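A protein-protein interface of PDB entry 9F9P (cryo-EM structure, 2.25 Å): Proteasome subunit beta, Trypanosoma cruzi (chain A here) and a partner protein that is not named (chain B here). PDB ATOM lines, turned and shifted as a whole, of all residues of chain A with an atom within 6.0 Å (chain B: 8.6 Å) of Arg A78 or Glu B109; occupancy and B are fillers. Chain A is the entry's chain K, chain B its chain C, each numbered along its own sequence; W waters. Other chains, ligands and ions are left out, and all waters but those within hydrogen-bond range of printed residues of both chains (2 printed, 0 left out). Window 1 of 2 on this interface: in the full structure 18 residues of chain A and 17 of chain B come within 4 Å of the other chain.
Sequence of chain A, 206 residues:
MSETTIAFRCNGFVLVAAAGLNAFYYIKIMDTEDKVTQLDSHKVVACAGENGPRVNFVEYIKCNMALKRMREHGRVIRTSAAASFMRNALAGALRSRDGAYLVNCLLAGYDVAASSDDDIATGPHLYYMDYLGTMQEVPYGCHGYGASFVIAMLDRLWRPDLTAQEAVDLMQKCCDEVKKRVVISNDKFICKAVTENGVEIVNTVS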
ATOM      1  N   LYS A  43      -8.570 -10.764 -16.279  1.00  0.00           N
ATOM      2  CA  LYS A  43      -8.640 -10.305 -17.656  1.00  0.00           C
ATOM      3  C   LYS A  43     -10.036  -9.861 -18.065  1.00  0.00           C
ATOM      4  O   LYS A  43     -10.979 -10.524 -17.675  1.00  0.00           O
ATOM      5  CB  LYS A  43      -8.283 -11.438 -18.601  1.00  0.00           C
ATOM      6  CG  LYS A  43      -6.807 -11.710 -18.687  1.00  0.00           C
ATOM      7  CD  LYS A  43      -6.451 -12.581 -19.869  1.00  0.00           C
ATOM      8  CE  LYS A  43      -5.830 -13.924 -19.565  1.00  0.00           C
ATOM      9  NZ  LYS A  43      -4.935 -13.893 -18.385  1.00  0.00           N
ATOM     10  N   LYS A  68      -8.285 -24.824 -22.508  1.00  0.00           N
ATOM     11  CA  LYS A  68      -6.847 -24.711 -22.329  1.00  0.00           C
ATOM     12  C   LYS A  68      -6.451 -24.672 -20.866  1.00  0.00           C
ATOM     13  O   LYS A  68      -5.364 -25.101 -20.556  1.00  0.00           O
ATOM     14  CB  LYS A  68      -6.290 -23.419 -22.929  1.00  0.00           C
ATOM     15  CG  LYS A  68      -4.821 -23.487 -23.264  1.00  0.00           C
ATOM     16  CD  LYS A  68      -4.122 -22.167 -23.400  1.00  0.00           C
ATOM     17  CE  LYS A  68      -2.635 -22.386 -23.609  1.00  0.00           C
ATOM     18  NZ  LYS A  68      -1.883 -21.111 -23.678  1.00  0.00           N
ATOM     19  N   GLU A  72      -3.989 -28.027 -18.356  1.00  0.00           N
ATOM     20  CA  GLU A  72      -2.793 -27.288 -17.957  1.00  0.00           C
ATOM     21  C   GLU A  72      -2.792 -27.014 -16.447  1.00  0.00           C
ATOM     22  O   GLU A  72      -2.125 -26.084 -15.991  1.00  0.00           O
ATOM     23  CB  GLU A  72      -2.685 -25.990 -18.763  1.00  0.00           C
ATOM     24  CG  GLU A  72      -1.261 -25.526 -19.017  1.00  0.00           C
ATOM     25  CD  GLU A  72      -1.058 -24.695 -20.282  1.00  0.00           C
ATOM     26  OE1 GLU A  72       0.015 -24.056 -20.405  1.00  0.00           O
ATOM     27  OE2 GLU A  72      -1.946 -24.702 -21.156  1.00  0.00           O
ATOM     28  N   VAL A  76      -3.238 -19.873 -14.737  1.00  0.00           N
ATOM     29  CA  VAL A  76      -3.644 -18.670 -15.444  1.00  0.00           C
ATOM     30  C   VAL A  76      -2.714 -18.469 -16.641  1.00  0.00           C
ATOM     31  O   VAL A  76      -1.493 -18.433 -16.511  1.00  0.00           O
ATOM     32  CB  VAL A  76      -3.631 -17.420 -14.535  1.00  0.00           C
ATOM     33  CG1 VAL A  76      -4.275 -16.228 -15.229  1.00  0.00           C
ATOM     34  CG2 VAL A  76      -4.293 -17.653 -13.176  1.00  0.00           C
ATOM     35  N   ILE A  77      -3.333 -18.281 -17.797  1.00  0.00           N
ATOM     36  CA  ILE A  77      -2.646 -18.033 -19.047  1.00  0.00           C
ATOM     37  C   ILE A  77      -2.205 -16.576 -19.133  1.00  0.00           C
ATOM     38  O   ILE A  77      -2.860 -15.694 -18.618  1.00  0.00           O
ATOM     39  CB  ILE A  77      -3.554 -18.497 -20.204  1.00  0.00           C
ATOM     40  CG1 ILE A  77      -3.638 -17.510 -21.361  1.00  0.00           C
ATOM     41  CG2 ILE A  77      -4.962 -18.868 -19.733  1.00  0.00           C
ATOM     42  CD1 ILE A  77      -4.121 -18.157 -22.651  1.00  0.00           C
ATOM     43  N   ARG A  78      -1.064 -16.314 -19.759  1.00  0.00           N
ATOM     44  CA  ARG A  78      -0.545 -14.963 -19.893  1.00  0.00           C
ATOM     45  C   ARG A  78      -1.375 -14.084 -20.829  1.00  0.00           C
ATOM     46  O   ARG A  78      -1.881 -14.549 -21.836  1.00  0.00           O
ATOM     47  CB  ARG A  78       0.786 -14.953 -20.627  1.00  0.00           C
ATOM     48  CG  ARG A  78       1.953 -15.577 -19.904  1.00  0.00           C
ATOM     49  CD  ARG A  78       3.026 -15.781 -20.978  1.00  0.00           C
ATOM     50  NE  ARG A  78       3.520 -14.507 -21.492  1.00  0.00           N
ATOM     51  CZ  ARG A  78       4.689 -13.964 -21.172  1.00  0.00           C
ATOM     52  NH1 ARG A  78       4.850 -12.658 -21.304  1.00  0.00           N
ATOM     53  NH2 ARG A  78       5.643 -14.703 -20.619  1.00  0.00           N
ATOM     54  N   THR A  79      -1.329 -12.770 -20.624  1.00  0.00           N
ATOM     55  CA  THR A  79      -2.173 -11.885 -21.424  1.00  0.00           C
ATOM     56  C   THR A  79      -1.745 -11.872 -22.897  1.00  0.00           C
ATOM     57  O   THR A  79      -2.603 -11.894 -23.767  1.00  0.00           O
ATOM     58  CB  THR A  79      -2.237 -10.474 -20.822  1.00  0.00           C
ATOM     59  OG1 THR A  79      -2.571 -10.567 -19.437  1.00  0.00           O
ATOM     60  CG2 THR A  79      -3.240  -9.604 -21.554  1.00  0.00           C
ATOM     61  N   SER A  80      -0.448 -11.935 -23.184  1.00  0.00           N
ATOM     62  CA  SER A  80       0.006 -11.951 -24.574  1.00  0.00           C
ATOM     63  C   SER A  80      -0.423 -13.206 -25.334  1.00  0.00           C
ATOM     64  O   SER A  80      -0.567 -13.161 -26.554  1.00  0.00           O
ATOM     65  CB  SER A  80       1.461 -11.790 -24.682  1.00  0.00           C
ATOM     66  OG  SER A  80       2.099 -12.803 -23.937  1.00  0.00           O
ATOM     67  N   ALA A  81      -0.657 -14.307 -24.629  1.00  0.00           N
ATOM     68  CA  ALA A  81      -1.074 -15.533 -25.296  1.00  0.00           C
ATOM     69  C   ALA A  81      -2.541 -15.509 -25.645  1.00  0.00           C
ATOM     70  O   ALA A  81      -2.917 -15.998 -26.708  1.00  0.00           O
ATOM     71  CB  ALA A  81      -0.777 -16.725 -24.404  1.00  0.00           C
ATOM     72  N   ALA A  82      -3.363 -14.965 -24.761  1.00  0.00           N
ATOM     73  CA  ALA A  82      -4.769 -14.701 -25.042  1.00  0.00           C
ATOM     74  C   ALA A  82      -4.979 -13.711 -26.177  1.00  0.00           C
ATOM     75  O   ALA A  82      -5.829 -13.937 -27.031  1.00  0.00           O
ATOM     76  CB  ALA A  82      -5.426 -14.189 -23.810  1.00  0.00           C
ATOM     77  N   ALA A  83      -4.141 -12.673 -26.237  1.00  0.00           N
ATOM     78  CA  ALA A  83      -4.192 -11.686 -27.312  1.00  0.00           C
ATOM     79  C   ALA A  83      -3.876 -12.320 -28.654  1.00  0.00           C
ATOM     80  O   ALA A  83      -4.520 -12.050 -29.631  1.00  0.00           O
ATOM     81  CB  ALA A  83      -3.190 -10.594 -27.055  1.00  0.00           C
ATOM     82  N   ASP A 111      -0.778  -9.777 -15.359  1.00  0.00           N
ATOM     83  CA  ASP A 111      -0.046 -11.032 -15.306  1.00  0.00           C
ATOM     84  C   ASP A 111       0.506 -11.297 -13.920  1.00  0.00           C
ATOM     85  O   ASP A 111       1.075 -10.426 -13.302  1.00  0.00           O
ATOM     86  CB  ASP A 111       1.121 -11.039 -16.289  1.00  0.00           C
ATOM     87  CG  ASP A 111       0.687 -11.285 -17.728  1.00  0.00           C
ATOM     88  OD1 ASP A 111      -0.447 -11.751 -17.941  1.00  0.00           O
ATOM     89  OD2 ASP A 111       1.486 -10.972 -18.635  1.00  0.00           O
ATOM     90  N   ILE A 120       8.600 -14.612 -15.381  1.00  0.00           N
ATOM     91  CA  ILE A 120       7.760 -13.655 -16.094  1.00  0.00           C
ATOM     92  C   ILE A 120       7.831 -12.321 -15.351  1.00  0.00           C
ATOM     93  O   ILE A 120       7.763 -12.294 -14.126  1.00  0.00           O
ATOM     94  CB  ILE A 120       6.295 -14.171 -16.201  1.00  0.00           C
ATOM     95  CG1 ILE A 120       5.465 -13.444 -17.269  1.00  0.00           C
ATOM     96  CG2 ILE A 120       5.566 -14.135 -14.852  1.00  0.00           C
ATOM     97  CD1 ILE A 120       3.994 -13.849 -17.307  1.00  0.00           C
ATOM     98  N   ALA A 121       7.945 -11.221 -16.102  1.00  0.00           N
ATOM     99  CA  ALA A 121       7.731  -9.894 -15.540  1.00  0.00           C
ATOM    100  C   ALA A 121       6.234  -9.671 -15.295  1.00  0.00           C
ATOM    101  O   ALA A 121       5.439  -9.610 -16.228  1.00  0.00           O
ATOM    102  CB  ALA A 121       8.316  -8.848 -16.462  1.00  0.00           C
ATOM    103  N   HIS B  77      13.162 -25.781 -25.735  1.00  0.00           N
ATOM    104  CA  HIS B  77      12.992 -26.146 -24.345  1.00  0.00           C
ATOM    105  C   HIS B  77      12.648 -27.629 -24.122  1.00  0.00           C
ATOM    106  O   HIS B  77      12.260 -27.971 -23.011  1.00  0.00           O
ATOM    107  CB  HIS B  77      11.874 -25.269 -23.745  1.00  0.00           C
ATOM    108  CG  HIS B  77      10.511 -25.515 -24.286  1.00  0.00           C
ATOM    109  ND1 HIS B  77      10.161 -25.265 -25.596  1.00  0.00           N
ATOM    110  CD2 HIS B  77       9.390 -25.999 -23.687  1.00  0.00           C
ATOM    111  CE1 HIS B  77       8.886 -25.645 -25.770  1.00  0.00           C
ATOM    112  NE2 HIS B  77       8.409 -26.116 -24.626  1.00  0.00           N
ATOM    113  N   SER B  99       3.627 -30.560 -33.709  1.00  0.00           N
ATOM    114  CA  SER B  99       2.717 -30.153 -32.655  1.00  0.00           C
ATOM    115  C   SER B  99       3.264 -29.000 -31.811  1.00  0.00           C
ATOM    116  O   SER B  99       2.544 -28.062 -31.493  1.00  0.00           O
ATOM    117  CB  SER B  99       2.463 -31.316 -31.767  1.00  0.00           C
ATOM    118  OG  SER B  99       1.483 -32.139 -32.304  1.00  0.00           O
ATOM    119  N   ALA B 100       4.520 -29.102 -31.407  1.00  0.00           N
ATOM    120  CA  ALA B 100       5.100 -28.128 -30.515  1.00  0.00           C
ATOM    121  C   ALA B 100       5.278 -26.794 -31.228  1.00  0.00           C
ATOM    122  O   ALA B 100       5.139 -25.762 -30.593  1.00  0.00           O
ATOM    123  CB  ALA B 100       6.419 -28.606 -29.976  1.00  0.00           C
ATOM    124  N   ASN B 101       5.562 -26.802 -32.520  1.00  0.00           N
ATOM    125  CA  ASN B 101       5.739 -25.564 -33.252  1.00  0.00           C
ATOM    126  C   ASN B 101       4.400 -25.001 -33.727  1.00  0.00           C
ATOM    127  O   ASN B 101       4.315 -23.829 -33.980  1.00  0.00           O
ATOM    128  CB  ASN B 101       6.804 -25.746 -34.355  1.00  0.00           C
ATOM    129  CG  ASN B 101       8.229 -25.764 -33.800  1.00  0.00           C
ATOM    130  OD1 ASN B 101       8.781 -24.696 -33.519  1.00  0.00           O
ATOM    131  ND2 ASN B 101       8.810 -26.942 -33.554  1.00  0.00           N
ATOM    132  N   ARG B 102       3.328 -25.773 -33.857  1.00  0.00           N
ATOM    133  CA  ARG B 102       2.030 -25.177 -34.100  1.00  0.00           C
ATOM    134  C   ARG B 102       1.500 -24.416 -32.891  1.00  0.00           C
ATOM    135  O   ARG B 102       0.865 -23.381 -33.041  1.00  0.00           O
ATOM    136  CB  ARG B 102       0.942 -26.190 -34.392  1.00  0.00           C
ATOM    137  CG  ARG B 102       0.762 -26.486 -35.857  1.00  0.00           C
ATOM    138  CD  ARG B 102      -0.610 -27.055 -36.175  1.00  0.00           C
ATOM    139  NE  ARG B 102      -0.453 -28.167 -37.121  1.00  0.00           N
ATOM    140  CZ  ARG B 102      -0.395 -29.442 -36.747  1.00  0.00           C
ATOM    141  NH1 ARG B 102      -0.582 -29.766 -35.477  1.00  0.00           N
ATOM    142  NH2 ARG B 102      -0.141 -30.390 -37.637  1.00  0.00           N
ATOM    143  N   HIS B 103       1.662 -24.972 -31.706  1.00  0.00           N
ATOM    144  CA  HIS B 103       1.313 -24.253 -30.507  1.00  0.00           C
ATOM    145  C   HIS B 103       1.992 -22.880 -30.490  1.00  0.00           C
ATOM    146  O   HIS B 103       1.383 -21.873 -30.190  1.00  0.00           O
ATOM    147  CB  HIS B 103       1.631 -25.110 -29.281  1.00  0.00           C
ATOM    148  CG  HIS B 103       1.157 -24.554 -27.987  1.00  0.00           C
ATOM    149  ND1 HIS B 103       1.882 -23.549 -27.364  1.00  0.00           N
ATOM    150  CD2 HIS B 103       0.127 -24.885 -27.163  1.00  0.00           C
ATOM    151  CE1 HIS B 103       1.287 -23.282 -26.196  1.00  0.00           C
ATOM    152  NE2 HIS B 103       0.193 -24.065 -26.060  1.00  0.00           N
ATOM    153  N   HIS B 104       3.266 -22.816 -30.801  1.00  0.00           N
ATOM    154  CA  HIS B 104       3.952 -21.546 -30.776  1.00  0.00           C
ATOM    155  C   HIS B 104       3.409 -20.588 -31.851  1.00  0.00           C
ATOM    156  O   HIS B 104       3.337 -19.398 -31.655  1.00  0.00           O
ATOM    157  CB  HIS B 104       5.451 -21.827 -30.861  1.00  0.00           C
ATOM    158  CG  HIS B 104       6.207 -20.575 -30.635  1.00  0.00           C
ATOM    159  ND1 HIS B 104       6.251 -19.577 -31.583  1.00  0.00           N
ATOM    160  CD2 HIS B 104       6.877 -20.141 -29.574  1.00  0.00           C
ATOM    161  CE1 HIS B 104       6.924 -18.554 -31.077  1.00  0.00           C
ATOM    162  NE2 HIS B 104       7.294 -18.869 -29.847  1.00  0.00           N
ATOM    163  N   TYR B 105       2.994 -21.090 -33.000  1.00  0.00           N
ATOM    164  CA  TYR B 105       2.331 -20.284 -33.995  1.00  0.00           C
ATOM    165  C   TYR B 105       1.024 -19.676 -33.477  1.00  0.00           C
ATOM    166  O   TYR B 105       0.717 -18.522 -33.776  1.00  0.00           O
ATOM    167  CB  TYR B 105       2.035 -21.135 -35.227  1.00  0.00           C
ATOM    168  CG  TYR B 105       1.171 -20.466 -36.261  1.00  0.00           C
ATOM    169  CD1 TYR B 105       1.684 -19.485 -37.096  1.00  0.00           C
ATOM    170  CD2 TYR B 105      -0.141 -20.839 -36.439  1.00  0.00           C
ATOM    171  CE1 TYR B 105       0.902 -18.856 -38.052  1.00  0.00           C
ATOM    172  CE2 TYR B 105      -0.955 -20.196 -37.365  1.00  0.00           C
ATOM    173  CZ  TYR B 105      -0.432 -19.199 -38.175  1.00  0.00           C
ATOM    174  OH  TYR B 105      -1.221 -18.553 -39.097  1.00  0.00           O
ATOM    175  N   THR B 106       0.214 -20.447 -32.756  1.00  0.00           N
ATOM    176  CA  THR B 106      -1.102 -20.005 -32.358  1.00  0.00           C
ATOM    177  C   THR B 106      -1.061 -19.074 -31.149  1.00  0.00           C
ATOM    178  O   THR B 106      -1.707 -18.043 -31.148  1.00  0.00           O
ATOM    179  CB  THR B 106      -1.977 -21.214 -32.048  1.00  0.00           C
ATOM    180  OG1 THR B 106      -2.187 -22.044 -33.185  1.00  0.00           O
ATOM    181  CG2 THR B 106      -3.321 -20.766 -31.523  1.00  0.00           C
ATOM    182  N   TYR B 107      -0.228 -19.362 -30.146  1.00  0.00           N
ATOM    183  CA  TYR B 107      -0.184 -18.585 -28.908  1.00  0.00           C
ATOM    184  C   TYR B 107       1.058 -17.727 -28.761  1.00  0.00           C
ATOM    185  O   TYR B 107       1.169 -16.989 -27.805  1.00  0.00           O
ATOM    186  CB  TYR B 107      -0.209 -19.535 -27.717  1.00  0.00           C
ATOM    187  CG  TYR B 107      -1.490 -20.302 -27.671  1.00  0.00           C
ATOM    188  CD1 TYR B 107      -2.669 -19.707 -27.235  1.00  0.00           C
ATOM    189  CD2 TYR B 107      -1.543 -21.621 -28.069  1.00  0.00           C
ATOM    190  CE1 TYR B 107      -3.858 -20.432 -27.190  1.00  0.00           C
ATOM    191  CE2 TYR B 107      -2.732 -22.344 -28.096  1.00  0.00           C
ATOM    192  CZ  TYR B 107      -3.905 -21.737 -27.680  1.00  0.00           C
ATOM    193  OH  TYR B 107      -5.071 -22.460 -27.691  1.00  0.00           O
ATOM    194  N   GLN B 108       2.026 -17.860 -29.667  1.00  0.00           N
ATOM    195  CA  GLN B 108       3.304 -17.169 -29.556  1.00  0.00           C
ATOM    196  C   GLN B 108       3.951 -17.396 -28.191  1.00  0.00           C
ATOM    197  O   GLN B 108       4.640 -16.534 -27.687  1.00  0.00           O
ATOM    198  CB  GLN B 108       3.137 -15.670 -29.878  1.00  0.00           C
ATOM    199  CG  GLN B 108       2.616 -15.386 -31.287  1.00  0.00           C
ATOM    200  CD  GLN B 108       3.651 -15.776 -32.315  1.00  0.00           C
ATOM    201  OE1 GLN B 108       4.836 -15.480 -32.153  1.00  0.00           O
ATOM    202  NE2 GLN B 108       3.239 -16.498 -33.356  1.00  0.00           N
ATOM    203  N   GLU B 109       3.781 -18.544 -27.575  1.00  0.00           N
ATOM    204  CA  GLU B 109       4.573 -18.880 -26.402  1.00  0.00           C
ATOM    205  C   GLU B 109       4.917 -20.361 -26.498  1.00  0.00           C
ATOM    206  O   GLU B 109       4.223 -21.069 -27.191  1.00  0.00           O
ATOM    207  CB  GLU B 109       3.816 -18.588 -25.098  1.00  0.00           C
ATOM    208  CG  GLU B 109       2.630 -19.505 -24.875  1.00  0.00           C
ATOM    209  CD  GLU B 109       1.984 -19.472 -23.495  1.00  0.00           C
ATOM    210  OE1 GLU B 109       0.848 -20.059 -23.352  1.00  0.00           O
ATOM    211  OE2 GLU B 109       2.617 -18.909 -22.546  1.00  0.00           O
ATOM    212  N   PRO B 110       5.902 -20.901 -25.741  1.00  0.00           N
ATOM    213  CA  PRO B 110       6.219 -22.330 -25.807  1.00  0.00           C
ATOM    214  C   PRO B 110       5.220 -23.289 -25.174  1.00  0.00           C
ATOM    215  O   PRO B 110       4.753 -23.050 -24.095  1.00  0.00           O
ATOM    216  CB  PRO B 110       7.544 -22.495 -25.057  1.00  0.00           C
ATOM    217  CG  PRO B 110       7.744 -21.206 -24.277  1.00  0.00           C
ATOM    218  CD  PRO B 110       6.712 -20.189 -24.746  1.00  0.00           C
ATOM    219  N   MET B 111       5.006 -24.432 -25.819  1.00  0.00           N
ATOM    220  CA  MET B 111       4.213 -25.537 -25.289  1.00  0.00           C
ATOM    221  C   MET B 111       4.769 -26.074 -23.986  1.00  0.00           C
ATOM    222  O   MET B 111       5.962 -26.325 -23.879  1.00  0.00           O
ATOM    223  CB  MET B 111       4.195 -26.712 -26.266  1.00  0.00           C
ATOM    224  CG  MET B 111       3.050 -27.684 -25.992  1.00  0.00           C
ATOM    225  SD  MET B 111       2.823 -28.883 -27.354  1.00  0.00           S
ATOM    226  CE  MET B 111       1.050 -28.897 -27.499  1.00  0.00           C
ATOM    227  N   ALA B 112       3.884 -26.296 -23.027  1.00  0.00           N
ATOM    228  CA  ALA B 112       4.224 -26.949 -21.768  1.00  0.00           C
ATOM    229  C   ALA B 112       4.744 -28.378 -21.963  1.00  0.00           C
ATOM    230  O   ALA B 112       4.318 -29.099 -22.853  1.00  0.00           O
ATOM    231  CB  ALA B 112       2.984 -26.964 -20.914  1.00  0.00           C
ATOM    232  N   ARG B 147       7.665 -22.736 -17.301  1.00  0.00           N
ATOM    233  CA  ARG B 147       7.436 -21.788 -16.207  1.00  0.00           C
ATOM    234  C   ARG B 147       6.455 -22.347 -15.175  1.00  0.00           C
ATOM    235  O   ARG B 147       6.360 -21.836 -14.088  1.00  0.00           O
ATOM    236  CB  ARG B 147       7.039 -20.405 -16.746  1.00  0.00           C
ATOM    237  CG  ARG B 147       5.669 -20.312 -17.398  1.00  0.00           C
ATOM    238  CD  ARG B 147       5.346 -18.915 -17.940  1.00  0.00           C
ATOM    239  NE  ARG B 147       3.941 -18.832 -18.355  1.00  0.00           N
ATOM    240  CZ  ARG B 147       2.945 -18.414 -17.568  1.00  0.00           C
ATOM    241  NH1 ARG B 147       1.680 -18.633 -17.900  1.00  0.00           N
ATOM    242  NH2 ARG B 147       3.220 -17.852 -16.402  1.00  0.00           N
ATOM    243  N   HIS B 148       5.779 -23.446 -15.470  1.00  0.00           N
ATOM    244  CA  HIS B 148       4.814 -23.993 -14.537  1.00  0.00           C
ATOM    245  C   HIS B 148       5.463 -24.917 -13.504  1.00  0.00           C
ATOM    246  O   HIS B 148       5.057 -24.901 -12.355  1.00  0.00           O
ATOM    247  CB  HIS B 148       3.692 -24.706 -15.300  1.00  0.00           C
ATOM    248  CG  HIS B 148       2.962 -23.879 -16.321  1.00  0.00           C
ATOM    249  ND1 HIS B 148       2.116 -22.833 -16.002  1.00  0.00           N
ATOM    250  CD2 HIS B 148       2.937 -23.964 -17.674  1.00  0.00           C
ATOM    251  CE1 HIS B 148       1.606 -22.313 -17.117  1.00  0.00           C
ATOM    252  NE2 HIS B 148       2.106 -22.978 -18.147  1.00  0.00           N
ATOM    253  N   TYR B 236       8.126  -3.563 -27.222  1.00  0.00           N
ATOM    254  CA  TYR B 236       7.372  -4.140 -26.114  1.00  0.00           C
ATOM    255  C   TYR B 236       7.778  -5.589 -25.842  1.00  0.00           C
ATOM    256  O   TYR B 236       7.152  -6.251 -25.015  1.00  0.00           O
ATOM    257  CB  TYR B 236       5.873  -4.068 -26.409  1.00  0.00           C
ATOM    258  CG  TYR B 236       5.280  -2.690 -26.332  1.00  0.00           C
ATOM    259  CD1 TYR B 236       4.788  -2.188 -25.134  1.00  0.00           C
ATOM    260  CD2 TYR B 236       5.230  -1.878 -27.456  1.00  0.00           C
ATOM    261  CE1 TYR B 236       4.236  -0.911 -25.055  1.00  0.00           C
ATOM    262  CE2 TYR B 236       4.699  -0.596 -27.388  1.00  0.00           C
ATOM    263  CZ  TYR B 236       4.201  -0.109 -26.183  1.00  0.00           C
ATOM    264  OH  TYR B 236       3.669   1.156 -26.136  1.00  0.00           O
ATOM    265  N   GLY B 237       8.836  -6.070 -26.516  1.00  0.00           N
ATOM    266  CA  GLY B 237       9.392  -7.390 -26.249  1.00  0.00           C
ATOM    267  C   GLY B 237      10.139  -7.445 -24.914  1.00  0.00           C
ATOM    268  O   GLY B 237      10.954  -6.580 -24.625  1.00  0.00           O
ATOM    269  N   VAL B 238       9.837  -8.468 -24.105  1.00  0.00           N
ATOM    270  CA  VAL B 238      10.486  -8.675 -22.816  1.00  0.00           C
ATOM    271  C   VAL B 238      10.990 -10.115 -22.774  1.00  0.00           C
ATOM    272  O   VAL B 238      10.178 -11.037 -22.788  1.00  0.00           O
ATOM    273  CB  VAL B 238       9.532  -8.392 -21.633  1.00  0.00           C
ATOM    274  CG1 VAL B 238      10.255  -8.465 -20.292  1.00  0.00           C
ATOM    275  CG2 VAL B 238       8.810  -7.055 -21.767  1.00  0.00           C
ATOM    276  N   LEU B 239      12.321 -10.288 -22.740  1.00  0.00           N
ATOM    277  CA  LEU B 239      12.942 -11.574 -22.441  1.00  0.00           C
ATOM    278  C   LEU B 239      13.289 -11.629 -20.956  1.00  0.00           C
ATOM    279  O   LEU B 239      13.394 -10.585 -20.316  1.00  0.00           O
ATOM    280  CB  LEU B 239      14.206 -11.764 -23.289  1.00  0.00           C
ATOM    281  CG  LEU B 239      14.003 -12.142 -24.761  1.00  0.00           C
ATOM    282  CD1 LEU B 239      15.346 -12.423 -25.429  1.00  0.00           C
ATOM    283  CD2 LEU B 239      13.074 -13.345 -24.917  1.00  0.00           C
ATOM    284  N   PRO B 240      13.464 -12.835 -20.357  1.00  0.00           N
ATOM    285  CA  PRO B 240      14.080 -12.975 -19.030  1.00  0.00           C
ATOM    286  C   PRO B 240      15.611 -13.069 -19.096  1.00  0.00           C
ATOM    287  O   PRO B 240      16.198 -12.946 -20.168  1.00  0.00           O
ATOM    288  CB  PRO B 240      13.440 -14.268 -18.478  1.00  0.00           C
ATOM    289  CG  PRO B 240      12.555 -14.814 -19.604  1.00  0.00           C
ATOM    290  CD  PRO B 240      13.017 -14.135 -20.876  1.00  0.00           C
HETATM  291  O   HOH W   1       2.617 -15.011 -25.750  1.00  0.00           O
HETATM  292  O   HOH W   2       0.650 -25.900 -23.172  1.00  0.00           O
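Printed residues of chain A that touch a printed residue of chain B: Lys A68, Glu A72, Val A76, Arg A78 and Ala A81.
Of the 22 printed residues of chain B, 4 touch a printed residue of chain A.
Hydrophobic or aromatic side chains of chain B within 4 Å of the printed part of chain A: Tyr B107 and His B148.
Among the printed residues, 8 pairs touch across the chains.
Among the printed residues, Asp or Glu carboxylates within 4 Å of a Lys or Arg side-chain nitrogen of the other chain: Lys A68 with Glu B109.
Water W1 lies within hydrogen-bond range of the side-chain hydroxyl (OG) of Ser A80 (2.9 Å), the backbone carbonyl oxygen (O) of Gln B108 (3.2 Å) and the backbone carbonyl oxygen (O) of Tyr B107 (3.2 Å).
Water W2 lies within hydrogen-bond range of the backbone NH of Ala B112, the side-chain carboxylate of Glu A72 and a ring nitrogen (NE2) of His B103.
Among the printed residues, merely in contact across the chains: Arg A78 with Glu B109, Arg A78 with Arg B147, Ala A81 with Tyr B107, Ala A81 with Glu B109 and Lys A68 with Tyr B107.
Arg A78 touches two residues of chain B.
Glu B109 touches just these residues of chain A: Lys A68, Arg A78 and Ala A81.
Printed residues of chain A within 4 Å of His B148: Glu A72.
Printed residues of chain B within 4 Å of Val A76: Arg B147.
Printed residues of chain B within 4 Å of Lys A68: Tyr B107 (3.9 Å) and Glu B109 (2.9 Å).
The nearest printed residue of chain B that does not touch Val A76 is His B148 (5.0 Å).
NE of Arg A78 lies within hydrogen-bond range of OG of Ser A80 (3.3 Å).
The backbone carbonyl oxygen of Glu B109 is in hydrogen-bond range of a ring nitrogen (ND1) of His B103, 3.4 Å away.
The side-chain amino group (NZ) of Lys A68 is in salt-bridge range of the side-chain carboxylate (OE1) of Glu B109, 2.9 Å away.
The side-chain carboxylate of Glu A72 lies within hydrogen-bond range of a ring nitrogen (NE2) of His B148 (3.3 Å).
The backbone carbonyl oxygen (O) of Val A76 lies within hydrogen-bond range of the guanidinium group (NH1) of Arg B147 (3.5 Å).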
